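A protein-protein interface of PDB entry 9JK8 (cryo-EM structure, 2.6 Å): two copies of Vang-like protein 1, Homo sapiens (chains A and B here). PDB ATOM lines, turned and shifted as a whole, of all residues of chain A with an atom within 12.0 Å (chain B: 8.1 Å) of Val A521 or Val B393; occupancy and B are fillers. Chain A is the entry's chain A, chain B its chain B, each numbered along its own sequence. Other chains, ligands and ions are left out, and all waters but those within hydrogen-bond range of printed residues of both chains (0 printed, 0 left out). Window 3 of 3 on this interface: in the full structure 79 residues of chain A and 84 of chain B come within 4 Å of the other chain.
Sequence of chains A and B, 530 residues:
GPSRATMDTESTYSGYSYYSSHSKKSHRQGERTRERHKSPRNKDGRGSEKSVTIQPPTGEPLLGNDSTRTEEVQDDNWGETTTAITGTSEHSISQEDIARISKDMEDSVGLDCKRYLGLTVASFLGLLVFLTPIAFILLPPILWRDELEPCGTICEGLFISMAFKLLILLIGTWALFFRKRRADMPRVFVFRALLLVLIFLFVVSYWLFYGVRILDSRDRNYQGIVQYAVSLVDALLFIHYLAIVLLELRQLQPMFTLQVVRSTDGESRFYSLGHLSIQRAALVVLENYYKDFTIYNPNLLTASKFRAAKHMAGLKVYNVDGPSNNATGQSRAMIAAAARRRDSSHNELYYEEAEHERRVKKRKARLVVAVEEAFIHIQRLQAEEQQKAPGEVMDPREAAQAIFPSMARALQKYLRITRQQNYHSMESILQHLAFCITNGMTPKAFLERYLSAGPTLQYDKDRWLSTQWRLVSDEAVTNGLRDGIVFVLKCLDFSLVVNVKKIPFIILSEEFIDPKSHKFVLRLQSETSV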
ATOM      1  N   ASP A 514       6.067   4.918  -4.691  1.00  0.00           N
ATOM      2  CA  ASP A 514       7.007   3.879  -4.348  1.00  0.00           C
ATOM      3  C   ASP A 514       8.073   4.451  -3.417  1.00  0.00           C
ATOM      4  O   ASP A 514       8.600   5.535  -3.678  1.00  0.00           O
ATOM      5  CB  ASP A 514       7.609   3.346  -5.642  1.00  0.00           C
ATOM      6  CG  ASP A 514       8.448   2.114  -5.443  1.00  0.00           C
ATOM      7  OD1 ASP A 514       8.371   1.498  -4.361  1.00  0.00           O
ATOM      8  OD2 ASP A 514       9.189   1.759  -6.379  1.00  0.00           O
ATOM      9  N   PRO A 515       8.390   3.775  -2.309  1.00  0.00           N
ATOM     10  CA  PRO A 515       9.566   4.173  -1.521  1.00  0.00           C
ATOM     11  C   PRO A 515      10.874   4.083  -2.297  1.00  0.00           C
ATOM     12  O   PRO A 515      11.881   4.628  -1.837  1.00  0.00           O
ATOM     13  CB  PRO A 515       9.542   3.202  -0.335  1.00  0.00           C
ATOM     14  CG  PRO A 515       8.103   2.796  -0.225  1.00  0.00           C
ATOM     15  CD  PRO A 515       7.595   2.734  -1.628  1.00  0.00           C
ATOM     16  N   LYS A 516      10.883   3.402  -3.447  1.00  0.00           N
ATOM     17  CA  LYS A 516      12.007   3.523  -4.369  1.00  0.00           C
ATOM     18  C   LYS A 516      12.042   4.887  -5.043  1.00  0.00           C
ATOM     19  O   LYS A 516      13.093   5.284  -5.553  1.00  0.00           O
ATOM     20  CB  LYS A 516      11.939   2.442  -5.447  1.00  0.00           C
ATOM     21  CG  LYS A 516      12.165   1.019  -4.975  1.00  0.00           C
ATOM     22  CD  LYS A 516      12.100   0.063  -6.159  1.00  0.00           C
ATOM     23  CE  LYS A 516      12.293  -1.383  -5.736  1.00  0.00           C
ATOM     24  NZ  LYS A 516      12.209  -2.309  -6.900  1.00  0.00           N
ATOM     25  N   SER A 517      10.917   5.601  -5.074  1.00  0.00           N
ATOM     26  CA  SER A 517      10.835   6.901  -5.727  1.00  0.00           C
ATOM     27  C   SER A 517      11.172   8.055  -4.794  1.00  0.00           C
ATOM     28  O   SER A 517      11.063   9.216  -5.203  1.00  0.00           O
ATOM     29  CB  SER A 517       9.437   7.110  -6.320  1.00  0.00           C
ATOM     30  OG  SER A 517       8.456   7.201  -5.302  1.00  0.00           O
ATOM     31  N   HIS A 518      11.575   7.771  -3.558  1.00  0.00           N
ATOM     32  CA  HIS A 518      12.040   8.800  -2.630  1.00  0.00           C
ATOM     33  C   HIS A 518      13.550   8.962  -2.668  1.00  0.00           C
ATOM     34  O   HIS A 518      14.183   9.264  -1.655  1.00  0.00           O
ATOM     35  CB  HIS A 518      11.562   8.485  -1.214  1.00  0.00           C
ATOM     36  CG  HIS A 518      10.077   8.554  -1.049  1.00  0.00           C
ATOM     37  ND1 HIS A 518       9.381   9.744  -1.087  1.00  0.00           N
ATOM     38  CD2 HIS A 518       9.154   7.585  -0.844  1.00  0.00           C
ATOM     39  CE1 HIS A 518       8.093   9.503  -0.914  1.00  0.00           C
ATOM     40  NE2 HIS A 518       7.929   8.201  -0.763  1.00  0.00           N
ATOM     41  N   LYS A 519      14.152   8.743  -3.835  1.00  0.00           N
ATOM     42  CA  LYS A 519      15.573   8.976  -4.014  1.00  0.00           C
ATOM     43  C   LYS A 519      15.845  10.473  -4.075  1.00  0.00           C
ATOM     44  O   LYS A 519      14.982  11.265  -4.465  1.00  0.00           O
ATOM     45  CB  LYS A 519      16.068   8.302  -5.294  1.00  0.00           C
ATOM     46  CG  LYS A 519      15.753   6.819  -5.360  1.00  0.00           C
ATOM     47  CD  LYS A 519      16.299   6.058  -4.165  1.00  0.00           C
ATOM     48  CE  LYS A 519      15.918   4.585  -4.239  1.00  0.00           C
ATOM     49  NZ  LYS A 519      16.405   3.933  -5.486  1.00  0.00           N
ATOM     50  N   PHE A 520      17.055  10.861  -3.681  1.00  0.00           N
ATOM     51  CA  PHE A 520      17.435  12.265  -3.675  1.00  0.00           C
ATOM     52  C   PHE A 520      18.903  12.396  -4.045  1.00  0.00           C
ATOM     53  O   PHE A 520      19.703  11.485  -3.815  1.00  0.00           O
ATOM     54  CB  PHE A 520      17.172  12.911  -2.307  1.00  0.00           C
ATOM     55  CG  PHE A 520      15.720  13.187  -2.040  1.00  0.00           C
ATOM     56  CD1 PHE A 520      15.129  14.356  -2.489  1.00  0.00           C
ATOM     57  CD2 PHE A 520      14.943  12.270  -1.354  1.00  0.00           C
ATOM     58  CE1 PHE A 520      13.793  14.609  -2.248  1.00  0.00           C
ATOM     59  CE2 PHE A 520      13.605  12.515  -1.114  1.00  0.00           C
ATOM     60  CZ  PHE A 520      13.030  13.686  -1.562  1.00  0.00           C
ATOM     61  N   VAL A 521      19.248  13.544  -4.623  1.00  0.00           N
ATOM     62  CA  VAL A 521      20.618  13.840  -5.010  1.00  0.00           C
ATOM     63  C   VAL A 521      21.036  15.155  -4.365  1.00  0.00           C
ATOM     64  O   VAL A 521      20.208  15.999  -4.013  1.00  0.00           O
ATOM     65  CB  VAL A 521      20.799  13.904  -6.542  1.00  0.00           C
ATOM     66  CG1 VAL A 521      20.512  12.548  -7.169  1.00  0.00           C
ATOM     67  CG2 VAL A 521      19.905  14.978  -7.141  1.00  0.00           C
ATOM     68  N   LEU A 522      22.349  15.315  -4.213  1.00  0.00           N
ATOM     69  CA  LEU A 522      22.926  16.488  -3.573  1.00  0.00           C
ATOM     70  C   LEU A 522      22.885  17.725  -4.464  1.00  0.00           C
ATOM     71  O   LEU A 522      23.183  18.826  -3.986  1.00  0.00           O
ATOM     72  CB  LEU A 522      24.367  16.173  -3.154  1.00  0.00           C
ATOM     73  CG  LEU A 522      25.161  17.131  -2.263  1.00  0.00           C
ATOM     74  CD1 LEU A 522      24.491  17.285  -0.909  1.00  0.00           C
ATOM     75  CD2 LEU A 522      26.585  16.622  -2.102  1.00  0.00           C
ATOM     76  N   ARG A 523      22.516  17.573  -5.733  1.00  0.00           N
ATOM     77  CA  ARG A 523      22.490  18.700  -6.654  1.00  0.00           C
ATOM     78  C   ARG A 523      21.375  19.679  -6.298  1.00  0.00           C
ATOM     79  O   ARG A 523      20.375  19.322  -5.670  1.00  0.00           O
ATOM     80  CB  ARG A 523      22.311  18.211  -8.092  1.00  0.00           C
ATOM     81  CG  ARG A 523      23.484  17.407  -8.625  1.00  0.00           C
ATOM     82  CD  ARG A 523      23.225  16.936 -10.045  1.00  0.00           C
ATOM     83  NE  ARG A 523      23.079  18.056 -10.968  1.00  0.00           N
ATOM     84  CZ  ARG A 523      24.088  18.652 -11.589  1.00  0.00           C
ATOM     85  NH1 ARG A 523      25.339  18.260 -11.411  1.00  0.00           N
ATOM     86  NH2 ARG A 523      23.836  19.668 -12.410  1.00  0.00           N
ATOM     87  N   LEU A 524      21.562  20.927  -6.716  1.00  0.00           N
ATOM     88  CA  LEU A 524      20.608  21.988  -6.446  1.00  0.00           C
ATOM     89  C   LEU A 524      19.334  21.792  -7.269  1.00  0.00           C
ATOM     90  O   LEU A 524      19.316  21.077  -8.275  1.00  0.00           O
ATOM     91  CB  LEU A 524      21.230  23.345  -6.770  1.00  0.00           C
ATOM     92  CG  LEU A 524      22.453  23.817  -5.982  1.00  0.00           C
ATOM     93  CD1 LEU A 524      23.027  25.078  -6.613  1.00  0.00           C
ATOM     94  CD2 LEU A 524      22.104  24.064  -4.525  1.00  0.00           C
ATOM     95  N   GLN A 525      18.257  22.440  -6.829  1.00  0.00           N
ATOM     96  CA  GLN A 525      17.014  22.440  -7.598  1.00  0.00           C
ATOM     97  C   GLN A 525      16.496  23.860  -7.816  1.00  0.00           C
ATOM     98  O   GLN A 525      16.589  24.713  -6.933  1.00  0.00           O
ATOM     99  CB  GLN A 525      15.934  21.595  -6.911  1.00  0.00           C
ATOM    100  CG  GLN A 525      15.432  22.141  -5.582  1.00  0.00           C
ATOM    101  CD  GLN A 525      14.297  21.314  -5.007  1.00  0.00           C
ATOM    102  OE1 GLN A 525      13.835  20.357  -5.630  1.00  0.00           O
ATOM    103  NE2 GLN A 525      13.837  21.684  -3.818  1.00  0.00           N
ATOM    104  N   PHE B 375      16.599  23.362   2.113  1.00  0.00           N
ATOM    105  CA  PHE B 375      15.744  22.561   1.241  1.00  0.00           C
ATOM    106  C   PHE B 375      16.023  22.802  -0.233  1.00  0.00           C
ATOM    107  O   PHE B 375      15.834  21.888  -1.045  1.00  0.00           O
ATOM    108  CB  PHE B 375      14.256  22.800   1.521  1.00  0.00           C
ATOM    109  CG  PHE B 375      13.740  22.090   2.739  1.00  0.00           C
ATOM    110  CD1 PHE B 375      14.604  21.436   3.597  1.00  0.00           C
ATOM    111  CD2 PHE B 375      12.380  22.014   2.982  1.00  0.00           C
ATOM    112  CE1 PHE B 375      14.124  20.767   4.702  1.00  0.00           C
ATOM    113  CE2 PHE B 375      11.893  21.342   4.085  1.00  0.00           C
ATOM    114  CZ  PHE B 375      12.767  20.717   4.946  1.00  0.00           C
ATOM    115  N   ILE B 376      16.466  24.005  -0.613  1.00  0.00           N
ATOM    116  CA  ILE B 376      16.768  24.225  -2.026  1.00  0.00           C
ATOM    117  C   ILE B 376      18.092  23.599  -2.441  1.00  0.00           C
ATOM    118  O   ILE B 376      18.397  23.559  -3.639  1.00  0.00           O
ATOM    119  CB  ILE B 376      16.745  25.729  -2.368  1.00  0.00           C
ATOM    120  CG1 ILE B 376      16.346  25.930  -3.830  1.00  0.00           C
ATOM    121  CG2 ILE B 376      18.099  26.367  -2.116  1.00  0.00           C
ATOM    122  CD1 ILE B 376      14.910  25.551  -4.128  1.00  0.00           C
ATOM    123  N   HIS B 377      18.880  23.087  -1.491  1.00  0.00           N
ATOM    124  CA  HIS B 377      20.143  22.432  -1.825  1.00  0.00           C
ATOM    125  C   HIS B 377      19.982  21.018  -2.369  1.00  0.00           C
ATOM    126  O   HIS B 377      20.982  20.436  -2.802  1.00  0.00           O
ATOM    127  CB  HIS B 377      21.077  22.389  -0.612  1.00  0.00           C
ATOM    128  CG  HIS B 377      21.921  23.614  -0.446  1.00  0.00           C
ATOM    129  ND1 HIS B 377      21.416  24.818  -0.003  1.00  0.00           N
ATOM    130  CD2 HIS B 377      23.241  23.819  -0.669  1.00  0.00           C
ATOM    131  CE1 HIS B 377      22.391  25.712   0.041  1.00  0.00           C
ATOM    132  NE2 HIS B 377      23.506  25.130  -0.358  1.00  0.00           N
ATOM    133  N   ILE B 378      18.783  20.441  -2.356  1.00  0.00           N
ATOM    134  CA  ILE B 378      18.582  19.085  -2.855  1.00  0.00           C
ATOM    135  C   ILE B 378      17.435  19.065  -3.856  1.00  0.00           C
ATOM    136  O   ILE B 378      16.410  19.727  -3.662  1.00  0.00           O
ATOM    137  CB  ILE B 378      18.329  18.072  -1.718  1.00  0.00           C
ATOM    138  CG1 ILE B 378      17.263  18.586  -0.749  1.00  0.00           C
ATOM    139  CG2 ILE B 378      19.632  17.731  -1.010  1.00  0.00           C
ATOM    140  CD1 ILE B 378      16.804  17.545   0.252  1.00  0.00           C
ATOM    141  N   GLN B 379      17.622  18.301  -4.927  1.00  0.00           N
ATOM    142  CA  GLN B 379      16.644  18.125  -5.989  1.00  0.00           C
ATOM    143  C   GLN B 379      15.941  16.783  -5.833  1.00  0.00           C
ATOM    144  O   GLN B 379      16.529  15.804  -5.364  1.00  0.00           O
ATOM    145  CB  GLN B 379      17.323  18.206  -7.359  1.00  0.00           C
ATOM    146  CG  GLN B 379      16.380  18.209  -8.547  1.00  0.00           C
ATOM    147  CD  GLN B 379      17.115  18.059  -9.864  1.00  0.00           C
ATOM    148  OE1 GLN B 379      18.338  17.908  -9.891  1.00  0.00           O
ATOM    149  NE2 GLN B 379      16.375  18.098 -10.965  1.00  0.00           N
ATOM    150  N   ARG B 380      14.665  16.746  -6.226  1.00  0.00           N
ATOM    151  CA  ARG B 380      13.888  15.516  -6.113  1.00  0.00           C
ATOM    152  C   ARG B 380      14.435  14.432  -7.035  1.00  0.00           C
ATOM    153  O   ARG B 380      14.914  13.390  -6.571  1.00  0.00           O
ATOM    154  CB  ARG B 380      12.416  15.802  -6.425  1.00  0.00           C
ATOM    155  CG  ARG B 380      11.529  14.567  -6.459  1.00  0.00           C
ATOM    156  CD  ARG B 380      11.489  13.880  -5.105  1.00  0.00           C
ATOM    157  NE  ARG B 380      10.627  12.703  -5.106  1.00  0.00           N
ATOM    158  CZ  ARG B 380       9.353  12.710  -4.740  1.00  0.00           C
ATOM    159  NH1 ARG B 380       8.753  13.819  -4.340  1.00  0.00           N
ATOM    160  NH2 ARG B 380       8.662  11.573  -4.777  1.00  0.00           N
ATOM    161  N   LEU B 381      14.394  14.676  -8.343  1.00  0.00           N
ATOM    162  CA  LEU B 381      14.831  13.714  -9.358  1.00  0.00           C
ATOM    163  C   LEU B 381      14.217  12.335  -9.115  1.00  0.00           C
ATOM    164  O   LEU B 381      13.542  11.784  -9.983  1.00  0.00           O
ATOM    165  CB  LEU B 381      16.365  13.629  -9.393  1.00  0.00           C
ATOM    166  CG  LEU B 381      17.057  12.815 -10.497  1.00  0.00           C
ATOM    167  CD1 LEU B 381      18.448  13.366 -10.752  1.00  0.00           C
ATOM    168  CD2 LEU B 381      17.150  11.333 -10.148  1.00  0.00           C
ATOM    169  N   GLU B 392      25.083  12.212  -6.308  1.00  0.00           N
ATOM    170  CA  GLU B 392      24.915  10.871  -5.762  1.00  0.00           C
ATOM    171  C   GLU B 392      23.493  10.648  -5.255  1.00  0.00           C
ATOM    172  O   GLU B 392      22.945  11.474  -4.527  1.00  0.00           O
ATOM    173  CB  GLU B 392      25.922  10.623  -4.634  1.00  0.00           C
ATOM    174  CG  GLU B 392      25.819   9.245  -3.999  1.00  0.00           C
ATOM    175  CD  GLU B 392      26.191   8.125  -4.952  1.00  0.00           C
ATOM    176  OE1 GLU B 392      27.010   8.363  -5.865  1.00  0.00           O
ATOM    177  OE2 GLU B 392      25.665   7.004  -4.788  1.00  0.00           O
ATOM    178  N   VAL B 393      22.904   9.523  -5.651  1.00  0.00           N
ATOM    179  CA  VAL B 393      21.539   9.189  -5.263  1.00  0.00           C
ATOM    180  C   VAL B 393      21.532   8.747  -3.807  1.00  0.00           C
ATOM    181  O   VAL B 393      22.328   7.891  -3.400  1.00  0.00           O
ATOM    182  CB  VAL B 393      20.967   8.097  -6.179  1.00  0.00           C
ATOM    183  CG1 VAL B 393      19.602   7.642  -5.684  1.00  0.00           C
ATOM    184  CG2 VAL B 393      20.882   8.601  -7.613  1.00  0.00           C
ATOM    185  N   MET B 394      20.632   9.328  -3.013  1.00  0.00           N
ATOM    186  CA  MET B 394      20.589   9.062  -1.584  1.00  0.00           C
ATOM    187  C   MET B 394      19.155   9.114  -1.080  1.00  0.00           C
ATOM    188  O   MET B 394      18.308   9.827  -1.621  1.00  0.00           O
ATOM    189  CB  MET B 394      21.468  10.060  -0.815  1.00  0.00           C
ATOM    190  CG  MET B 394      21.016  11.507  -0.924  1.00  0.00           C
ATOM    191  SD  MET B 394      22.226  12.652  -0.229  1.00  0.00           S
ATOM    192  CE  MET B 394      21.635  14.210  -0.885  1.00  0.00           C
ATOM    193  N   ASP B 395      18.899   8.336  -0.026  1.00  0.00           N
ATOM    194  CA  ASP B 395      17.599   8.285   0.619  1.00  0.00           C
ATOM    195  C   ASP B 395      17.367   9.555   1.439  1.00  0.00           C
ATOM    196  O   ASP B 395      18.303  10.311   1.710  1.00  0.00           O
ATOM    197  CB  ASP B 395      17.497   7.019   1.474  1.00  0.00           C
ATOM    198  CG  ASP B 395      18.508   6.984   2.611  1.00  0.00           C
ATOM    199  OD1 ASP B 395      19.329   7.916   2.733  1.00  0.00           O
ATOM    200  OD2 ASP B 395      18.482   6.005   3.386  1.00  0.00           O
ATOM    201  N   PRO B 396      16.117   9.832   1.830  1.00  0.00           N
ATOM    202  CA  PRO B 396      15.848  11.062   2.597  1.00  0.00           C
ATOM    203  C   PRO B 396      16.582  11.147   3.924  1.00  0.00           C
ATOM    204  O   PRO B 396      16.747  12.257   4.439  1.00  0.00           O
ATOM    205  CB  PRO B 396      14.327  11.023   2.801  1.00  0.00           C
ATOM    206  CG  PRO B 396      13.824  10.211   1.663  1.00  0.00           C
ATOM    207  CD  PRO B 396      14.866   9.151   1.448  1.00  0.00           C
ATOM    208  N   GLU B 398      19.877  10.285   4.345  1.00  0.00           N
ATOM    209  CA  GLU B 398      21.144  10.894   3.964  1.00  0.00           C
ATOM    210  C   GLU B 398      20.945  12.295   3.401  1.00  0.00           C
ATOM    211  O   GLU B 398      21.818  13.149   3.566  1.00  0.00           O
ATOM    212  CB  GLU B 398      21.882  10.001   2.967  1.00  0.00           C
ATOM    213  CG  GLU B 398      22.434   8.728   3.596  1.00  0.00           C
ATOM    214  CD  GLU B 398      23.104   7.811   2.591  1.00  0.00           C
ATOM    215  OE1 GLU B 398      23.029   8.100   1.378  1.00  0.00           O
ATOM    216  OE2 GLU B 398      23.708   6.804   3.017  1.00  0.00           O
ATOM    217  N   ALA B 399      19.807  12.561   2.755  1.00  0.00           N
ATOM    218  CA  ALA B 399      19.510  13.925   2.325  1.00  0.00           C
ATOM    219  C   ALA B 399      19.348  14.858   3.520  1.00  0.00           C
ATOM    220  O   ALA B 399      19.846  15.995   3.506  1.00  0.00           O
ATOM    221  CB  ALA B 399      18.251  13.939   1.458  1.00  0.00           C
ATOM    222  N   ALA B 402      22.653  15.523   4.894  1.00  0.00           N
ATOM    223  CA  ALA B 402      23.431  16.377   4.005  1.00  0.00           C
ATOM    224  C   ALA B 402      23.036  17.842   4.137  1.00  0.00           C
ATOM    225  O   ALA B 402      23.900  18.724   4.082  1.00  0.00           O
ATOM    226  CB  ALA B 402      23.269  15.909   2.559  1.00  0.00           C
ATOM    227  N   ILE B 403      21.742  18.127   4.301  1.00  0.00           N
ATOM    228  CA  ILE B 403      21.286  19.517   4.356  1.00  0.00           C
ATOM    229  C   ILE B 403      21.155  20.058   5.775  1.00  0.00           C
ATOM    230  O   ILE B 403      20.899  21.262   5.939  1.00  0.00           O
ATOM    231  CB  ILE B 403      19.948  19.708   3.611  1.00  0.00           C
ATOM    232  CG1 ILE B 403      18.814  18.981   4.333  1.00  0.00           C
ATOM    233  CG2 ILE B 403      20.069  19.236   2.176  1.00  0.00           C
ATOM    234  CD1 ILE B 403      17.444  19.332   3.801  1.00  0.00           C
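The backbone carbonyl oxygen (O) of Ser A517 is in hydrogen-bond range of the guanidinium group (NH2) of Arg B380 (3.4 Å).
The backbone carbonyl oxygen of Phe A520 lies within hydrogen-bond range of the backbone NH of Met B394, 2.5 Å away.
The backbone carbonyl oxygen of Arg A523 sits at hydrogen-bond distance from the backbone NH of Gln B379 (3.0 Å).
The side-chain amide nitrogen (NE2) of Gln A525 is in hydrogen-bond range of the backbone carbonyl oxygen (O) of Phe B375, 3.4 Å away.
N of Gln A525 is in hydrogen-bond range of O of Ile B376.
The backbone carbonyl oxygen (O) of Ile B378 lies close to the side-chain amide nitrogen (NE2) of Gln A525, 3.2 Å away.
The backbone carbonyl oxygen of Arg B380 sits close to the backbone carbonyl oxygen of Lys A519 (3.0 Å).
O of Phe A520 sits close to O of Glu B392 (3.3 Å).
The backbone carbonyl oxygen (O) of Leu A522 sits close to the backbone carbonyl oxygen (O) of His B377, at 3.0 Å.
The backbone carbonyl oxygen of Arg A523 lies close to the backbone carbonyl oxygen of His B377.
The backbone NH (N) of Asp A514 lies close to the side-chain hydroxyl (OG) of Ser A517 (3.4 Å).
Val B393 touches Lys A519.
Phe A520 touches Gln B379 (CD1 to O, 3.5 Å).
Phe A520 touches Val B393.
Phe A520 touches Pro B396 (CE2 to CG, 3.6 Å).
N of Gln B379 touches O of Val A521, at 3.6 Å.
Val A521 touches Met B394 (C to CE, 3.7 Å).
Met B394 touches Leu A522.
CA of Ile B378 touches O of Arg A523, 3.3 Å away.
Leu A524 touches Ile B376 (CD2 to O, 3.8 Å).
Gln B379 touches Leu A524.
Of the printed residues of chain B, Val A521 touches Ile B378 (3.5 Å), Gln B379 (3.6 Å), Glu B392 (3.4 Å), Val B393 (3.99 Å) and Met B394 (3.7 Å).
Of the printed residues of chain A, Val B393 touches Lys A519 (3.6 Å), Phe A520 (3.3 Å) and Val A521 (3.99 Å).
Ile B378 touches three residues of chain A.
No residue of chain A comes within 4 Å of Leu B381.
Of chain A, only Phe A520 (3.3 Å), Val A521 (3.4 Å) and Leu A522 (3.9 Å) come within 4 Å of Glu B392.
Of the printed residues of chain A, Met B394 touches Lys A519, Phe A520, Val A521 and Leu A522.
No residue of chain A comes within 4 Å of Ala B399.
Of the printed residues of chain A, Ala B402 touches Leu A522 (3.9 Å).
Of the printed residues of chain B, Ser A517 touches Arg B380.
Of the printed residues of chain A, Pro B396 touches His A518 and Phe A520.
The nearest printed residue of chain B that does not touch Val A521 is Leu B381 (4.2 Å).
Of the 12 printed residues of chain A, 9 touch a printed residue of chain B.
Printed residues of chain A that touch a printed residue of chain B: Ser A517, His A518, Lys A519, Phe A520, Val A521, Leu A522, Arg A523, Leu A524 and Gln A525.
Among the printed residues, no Asp or Glu carboxylate lies within 4 Å of a Lys or Arg side-chain nitrogen of the other chain.
No position is printed for both chains.
Of the 31 pairs that touch across the chains among the printed residues, none has its exchanged pair printed and touching as well.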
